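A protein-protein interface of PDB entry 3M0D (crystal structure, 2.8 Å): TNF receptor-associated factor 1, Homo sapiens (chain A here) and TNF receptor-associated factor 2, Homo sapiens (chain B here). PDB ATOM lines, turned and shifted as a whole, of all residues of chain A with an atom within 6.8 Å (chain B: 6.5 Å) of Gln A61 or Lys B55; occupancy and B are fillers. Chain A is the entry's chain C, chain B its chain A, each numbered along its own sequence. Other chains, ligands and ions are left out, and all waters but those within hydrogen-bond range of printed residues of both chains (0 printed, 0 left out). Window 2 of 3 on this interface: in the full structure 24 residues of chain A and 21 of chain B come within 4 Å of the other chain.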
ATOM      1  N   GLU A  54      -0.780 -29.613  15.919  1.00  0.00           N
ATOM      2  CA  GLU A  54       0.635 -29.961  15.891  1.00  0.00           C
ATOM      3  C   GLU A  54       0.840 -31.248  15.108  1.00  0.00           C
ATOM      4  O   GLU A  54       1.769 -31.350  14.312  1.00  0.00           O
ATOM      5  CB  GLU A  54       1.205 -30.100  17.296  1.00  0.00           C
ATOM      6  CG  GLU A  54       1.161 -28.810  18.086  1.00  0.00           C
ATOM      7  CD  GLU A  54       1.666 -28.944  19.530  1.00  0.00           C
ATOM      8  OE1 GLU A  54       1.469 -30.015  20.172  1.00  0.00           O
ATOM      9  OE2 GLU A  54       2.252 -27.947  20.024  1.00  0.00           O
ATOM     10  N   ARG A  56      -1.269 -32.731  12.801  1.00  0.00           N
ATOM     11  CA  ARG A  56      -1.526 -32.407  11.403  1.00  0.00           C
ATOM     12  C   ARG A  56      -0.339 -31.747  10.736  1.00  0.00           C
ATOM     13  O   ARG A  56      -0.040 -32.022   9.564  1.00  0.00           O
ATOM     14  CB  ARG A  56      -2.713 -31.464  11.276  1.00  0.00           C
ATOM     15  CG  ARG A  56      -4.046 -32.150  11.349  1.00  0.00           C
ATOM     16  CD  ARG A  56      -5.164 -31.137  11.477  1.00  0.00           C
ATOM     17  NE  ARG A  56      -5.575 -30.580  10.191  1.00  0.00           N
ATOM     18  CZ  ARG A  56      -6.503 -29.634  10.055  1.00  0.00           C
ATOM     19  NH1 ARG A  56      -6.836 -29.186   8.849  1.00  0.00           N
ATOM     20  NH2 ARG A  56      -7.106 -29.134  11.131  1.00  0.00           N
ATOM     21  N   VAL A  57       0.318 -30.856  11.477  1.00  0.00           N
ATOM     22  CA  VAL A  57       1.450 -30.071  10.956  1.00  0.00           C
ATOM     23  C   VAL A  57       2.753 -30.858  10.864  1.00  0.00           C
ATOM     24  O   VAL A  57       3.513 -30.691   9.915  1.00  0.00           O
ATOM     25  CB  VAL A  57       1.712 -28.787  11.778  1.00  0.00           C
ATOM     26  CG1 VAL A  57       3.182 -28.374  11.690  1.00  0.00           C
ATOM     27  CG2 VAL A  57       0.800 -27.653  11.314  1.00  0.00           C
ATOM     28  N   VAL A  58       3.020 -31.696  11.862  1.00  0.00           N
ATOM     29  CA  VAL A  58       4.140 -32.621  11.784  1.00  0.00           C
ATOM     30  C   VAL A  58       3.980 -33.520  10.540  1.00  0.00           C
ATOM     31  O   VAL A  58       4.944 -33.775   9.817  1.00  0.00           O
ATOM     32  CB  VAL A  58       4.283 -33.444  13.092  1.00  0.00           C
ATOM     33  CG1 VAL A  58       4.538 -34.927  12.789  1.00  0.00           C
ATOM     34  CG2 VAL A  58       5.380 -32.846  13.964  1.00  0.00           C
ATOM     35  N   GLU A  59       2.752 -33.961  10.279  1.00  0.00           N
ATOM     36  CA  GLU A  59       2.448 -34.740   9.081  1.00  0.00           C
ATOM     37  C   GLU A  59       2.923 -34.031   7.826  1.00  0.00           C
ATOM     38  O   GLU A  59       3.597 -34.620   6.987  1.00  0.00           O
ATOM     39  CB  GLU A  59       0.949 -34.995   8.962  1.00  0.00           C
ATOM     40  CG  GLU A  59       0.621 -36.428   8.631  1.00  0.00           C
ATOM     41  CD  GLU A  59       1.072 -37.373   9.729  1.00  0.00           C
ATOM     42  OE1 GLU A  59       0.942 -37.005  10.923  1.00  0.00           O
ATOM     43  OE2 GLU A  59       1.562 -38.476   9.394  1.00  0.00           O
ATOM     44  N   LEU A  60       2.551 -32.766   7.702  1.00  0.00           N
ATOM     45  CA  LEU A  60       2.942 -31.968   6.555  1.00  0.00           C
ATOM     46  C   LEU A  60       4.447 -31.806   6.453  1.00  0.00           C
ATOM     47  O   LEU A  60       5.000 -31.822   5.354  1.00  0.00           O
ATOM     48  CB  LEU A  60       2.275 -30.602   6.600  1.00  0.00           C
ATOM     49  CG  LEU A  60       0.900 -30.572   5.938  1.00  0.00           C
ATOM     50  CD1 LEU A  60       0.003 -31.659   6.534  1.00  0.00           C
ATOM     51  CD2 LEU A  60       0.278 -29.191   6.081  1.00  0.00           C
ATOM     52  N   GLN A  61       5.121 -31.657   7.590  1.00  0.00           N
ATOM     53  CA  GLN A  61       6.582 -31.566   7.589  1.00  0.00           C
ATOM     54  C   GLN A  61       7.228 -32.807   6.969  1.00  0.00           C
ATOM     55  O   GLN A  61       8.255 -32.712   6.302  1.00  0.00           O
ATOM     56  CB  GLN A  61       7.117 -31.371   9.011  1.00  0.00           C
ATOM     57  CG  GLN A  61       6.963 -29.950   9.560  1.00  0.00           C
ATOM     58  CD  GLN A  61       7.335 -29.833  11.042  1.00  0.00           C
ATOM     59  OE1 GLN A  61       6.971 -30.683  11.868  1.00  0.00           O
ATOM     60  NE2 GLN A  61       8.060 -28.771  11.381  1.00  0.00           N
ATOM     61  N   GLN A  62       6.609 -33.964   7.185  1.00  0.00           N
ATOM     62  CA  GLN A  62       7.219 -35.236   6.816  1.00  0.00           C
ATOM     63  C   GLN A  62       6.822 -35.795   5.447  1.00  0.00           C
ATOM     64  O   GLN A  62       7.430 -36.759   4.971  1.00  0.00           O
ATOM     65  CB  GLN A  62       6.979 -36.273   7.909  1.00  0.00           C
ATOM     66  CG  GLN A  62       7.756 -35.995   9.181  1.00  0.00           C
ATOM     67  CD  GLN A  62       7.427 -36.988  10.286  1.00  0.00           C
ATOM     68  OE1 GLN A  62       6.607 -37.891  10.099  1.00  0.00           O
ATOM     69  NE2 GLN A  62       8.065 -36.825  11.445  1.00  0.00           N
ATOM     70  N   THR A  63       5.805 -35.212   4.818  1.00  0.00           N
ATOM     71  CA  THR A  63       5.591 -35.458   3.395  1.00  0.00           C
ATOM     72  C   THR A  63       6.024 -34.240   2.597  1.00  0.00           C
ATOM     73  O   THR A  63       5.294 -33.765   1.746  1.00  0.00           O
ATOM     74  CB  THR A  63       4.143 -35.888   3.029  1.00  0.00           C
ATOM     75  OG1 THR A  63       3.201 -34.924   3.507  1.00  0.00           O
ATOM     76  CG2 THR A  63       3.818 -37.271   3.615  1.00  0.00           C
ATOM     77  N   LEU A  64       7.216 -33.741   2.918  1.00  0.00           N
ATOM     78  CA  LEU A  64       7.893 -32.693   2.163  1.00  0.00           C
ATOM     79  C   LEU A  64       9.374 -33.014   2.076  1.00  0.00           C
ATOM     80  O   LEU A  64      10.178 -32.174   1.670  1.00  0.00           O
ATOM     81  CB  LEU A  64       7.720 -31.316   2.810  1.00  0.00           C
ATOM     82  CG  LEU A  64       6.462 -30.495   2.499  1.00  0.00           C
ATOM     83  CD1 LEU A  64       6.762 -28.997   2.536  1.00  0.00           C
ATOM     84  CD2 LEU A  64       5.871 -30.869   1.159  1.00  0.00           C
ATOM     85  N   GLU B  50       2.762 -19.940  19.055  1.00  0.00           N
ATOM     86  CA  GLU B  50       3.828 -19.246  18.362  1.00  0.00           C
ATOM     87  C   GLU B  50       4.655 -20.262  17.595  1.00  0.00           C
ATOM     88  O   GLU B  50       5.140 -19.984  16.505  1.00  0.00           O
ATOM     89  CB  GLU B  50       4.699 -18.452  19.339  1.00  0.00           C
ATOM     90  CG  GLU B  50       4.087 -17.115  19.738  1.00  0.00           C
ATOM     91  CD  GLU B  50       4.833 -16.421  20.878  1.00  0.00           C
ATOM     92  OE1 GLU B  50       6.087 -16.348  20.808  1.00  0.00           O
ATOM     93  OE2 GLU B  50       4.153 -15.951  21.834  1.00  0.00           O
ATOM     94  N   ALA B  51       4.804 -21.445  18.178  1.00  0.00           N
ATOM     95  CA  ALA B  51       5.598 -22.504  17.584  1.00  0.00           C
ATOM     96  C   ALA B  51       4.896 -23.062  16.352  1.00  0.00           C
ATOM     97  O   ALA B  51       5.535 -23.336  15.331  1.00  0.00           O
ATOM     98  CB  ALA B  51       5.851 -23.594  18.598  1.00  0.00           C
ATOM     99  N   LEU B  52       3.581 -23.231  16.448  1.00  0.00           N
ATOM    100  CA  LEU B  52       2.789 -23.591  15.282  1.00  0.00           C
ATOM    101  C   LEU B  52       2.838 -22.524  14.184  1.00  0.00           C
ATOM    102  O   LEU B  52       3.158 -22.829  13.037  1.00  0.00           O
ATOM    103  CB  LEU B  52       1.345 -23.870  15.681  1.00  0.00           C
ATOM    104  CG  LEU B  52       1.165 -25.333  16.049  1.00  0.00           C
ATOM    105  CD1 LEU B  52      -0.277 -25.676  16.392  1.00  0.00           C
ATOM    106  CD2 LEU B  52       1.672 -26.167  14.900  1.00  0.00           C
ATOM    107  N   SER B  53       2.531 -21.277  14.534  1.00  0.00           N
ATOM    108  CA  SER B  53       2.509 -20.214  13.535  1.00  0.00           C
ATOM    109  C   SER B  53       3.866 -20.105  12.849  1.00  0.00           C
ATOM    110  O   SER B  53       3.964 -19.715  11.685  1.00  0.00           O
ATOM    111  CB  SER B  53       2.135 -18.875  14.161  1.00  0.00           C
ATOM    112  OG  SER B  53       3.290 -18.198  14.642  1.00  0.00           O
ATOM    113  N   SER B  54       4.911 -20.443  13.591  1.00  0.00           N
ATOM    114  CA  SER B  54       6.262 -20.389  13.075  1.00  0.00           C
ATOM    115  C   SER B  54       6.476 -21.543  12.074  1.00  0.00           C
ATOM    116  O   SER B  54       7.083 -21.359  11.008  1.00  0.00           O
ATOM    117  CB  SER B  54       7.258 -20.461  14.237  1.00  0.00           C
ATOM    118  OG  SER B  54       8.516 -19.917  13.890  1.00  0.00           O
ATOM    119  N   LYS B  55       5.962 -22.725  12.407  1.00  0.00           N
ATOM    120  CA  LYS B  55       6.108 -23.886  11.527  1.00  0.00           C
ATOM    121  C   LYS B  55       5.197 -23.801  10.307  1.00  0.00           C
ATOM    122  O   LYS B  55       5.491 -24.386   9.260  1.00  0.00           O
ATOM    123  CB  LYS B  55       5.834 -25.193  12.274  1.00  0.00           C
ATOM    124  CG  LYS B  55       6.827 -25.528  13.375  1.00  0.00           C
ATOM    125  CD  LYS B  55       6.410 -26.802  14.110  1.00  0.00           C
ATOM    126  CE  LYS B  55       7.304 -27.093  15.309  1.00  0.00           C
ATOM    127  NZ  LYS B  55       8.645 -27.608  14.903  1.00  0.00           N
ATOM    128  N   VAL B  56       4.082 -23.089  10.443  1.00  0.00           N
ATOM    129  CA  VAL B  56       3.151 -22.935   9.330  1.00  0.00           C
ATOM    130  C   VAL B  56       3.675 -21.923   8.309  1.00  0.00           C
ATOM    131  O   VAL B  56       3.552 -22.143   7.104  1.00  0.00           O
ATOM    132  CB  VAL B  56       1.707 -22.625   9.809  1.00  0.00           C
ATOM    133  CG1 VAL B  56       0.837 -22.138   8.674  1.00  0.00           C
ATOM    134  CG2 VAL B  56       1.085 -23.864  10.406  1.00  0.00           C
ATOM    135  N   GLN B  57       4.305 -20.848   8.784  1.00  0.00           N
ATOM    136  CA  GLN B  57       4.953 -19.901   7.885  1.00  0.00           C
ATOM    137  C   GLN B  57       6.076 -20.559   7.070  1.00  0.00           C
ATOM    138  O   GLN B  57       6.118 -20.418   5.853  1.00  0.00           O
ATOM    139  CB  GLN B  57       5.486 -18.690   8.650  1.00  0.00           C
ATOM    140  CG  GLN B  57       5.927 -17.546   7.731  1.00  0.00           C
ATOM    141  CD  GLN B  57       6.376 -16.291   8.473  1.00  0.00           C
ATOM    142  OE1 GLN B  57       7.184 -16.356   9.401  1.00  0.00           O
ATOM    143  NE2 GLN B  57       5.858 -15.140   8.052  1.00  0.00           N
ATOM    144  N   GLN B  58       6.974 -21.282   7.740  1.00  0.00           N
ATOM    145  CA  GLN B  58       8.068 -21.994   7.071  1.00  0.00           C
ATOM    146  C   GLN B  58       7.559 -22.866   5.915  1.00  0.00           C
ATOM    147  O   GLN B  58       8.153 -22.881   4.825  1.00  0.00           O
ATOM    148  CB  GLN B  58       8.868 -22.834   8.085  1.00  0.00           C
ATOM    149  CG  GLN B  58       9.657 -24.012   7.484  1.00  0.00           C
ATOM    150  CD  GLN B  58      10.923 -23.591   6.740  1.00  0.00           C
ATOM    151  OE1 GLN B  58      11.628 -22.672   7.158  1.00  0.00           O
ATOM    152  NE2 GLN B  58      11.215 -24.268   5.630  1.00  0.00           N
ATOM    153  N   LEU B  59       6.460 -23.582   6.162  1.00  0.00           N
ATOM    154  CA  LEU B  59       5.815 -24.425   5.150  1.00  0.00           C
ATOM    155  C   LEU B  59       5.249 -23.634   3.966  1.00  0.00           C
ATOM    156  O   LEU B  59       5.550 -23.920   2.805  1.00  0.00           O
ATOM    157  CB  LEU B  59       4.678 -25.237   5.774  1.00  0.00           C
ATOM    158  CG  LEU B  59       5.010 -26.338   6.771  1.00  0.00           C
ATOM    159  CD1 LEU B  59       3.735 -26.972   7.311  1.00  0.00           C
ATOM    160  CD2 LEU B  59       5.909 -27.387   6.140  1.00  0.00           C
ATOM    161  N   GLU B  60       4.405 -22.657   4.264  1.00  0.00           N
ATOM    162  CA  GLU B  60       3.845 -21.800   3.231  1.00  0.00           C
ATOM    163  C   GLU B  60       4.911 -21.235   2.275  1.00  0.00           C
ATOM    164  O   GLU B  60       4.711 -21.232   1.059  1.00  0.00           O
ATOM    165  CB  GLU B  60       3.054 -20.673   3.890  1.00  0.00           C
ATOM    166  CG  GLU B  60       1.964 -21.206   4.805  1.00  0.00           C
ATOM    167  CD  GLU B  60       0.997 -20.142   5.317  1.00  0.00           C
ATOM    168  OE1 GLU B  60       1.461 -19.070   5.778  1.00  0.00           O
ATOM    169  OE2 GLU B  60      -0.232 -20.401   5.257  1.00  0.00           O
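Among the printed residues, pairs that only touch across the chains: Gln A61 with Lys B55, Glu A54 with Leu B52, Val A57 with Val B56, Leu A60 with Leu B59 and Val A57 with Leu B52.
Of chain B, only Lys B55 comes within 4 Å of Gln A61.
Of the printed residues of chain B, Glu A54 touches Leu B52 (3.8 Å).
Of the printed residues of chain B, Leu A60 touches Leu B59.
Gln B57 touches none of the printed residues of chain A.
The nearest residue of chain A that does not touch Lys B55 is Val A57 (4.2 Å).
The nearest printed residue of chain A that does not touch Leu B52 is Val A58 (6.5 Å).
Printed residues of chain A that touch a printed residue of chain B: Glu A54, Val A57, Leu A60 and Gln A61.
Hydrophobic or aromatic side chains of chain A within 4 Å of the printed part of chain B: Val A57 and Leu A60.
Along chain A the printed residues that touch a printed residue of chain B span positions 54 to 61.
Printed residues of chain B that touch a printed residue of chain A: Leu B52, Lys B55, Val B56 and Leu B59.
Hydrophobic or aromatic side chains of chain B within 4 Å of the printed part of chain A: Leu B52, Val B56 and Leu B59.
Among the printed residues, 5 pairs touch across the chains.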
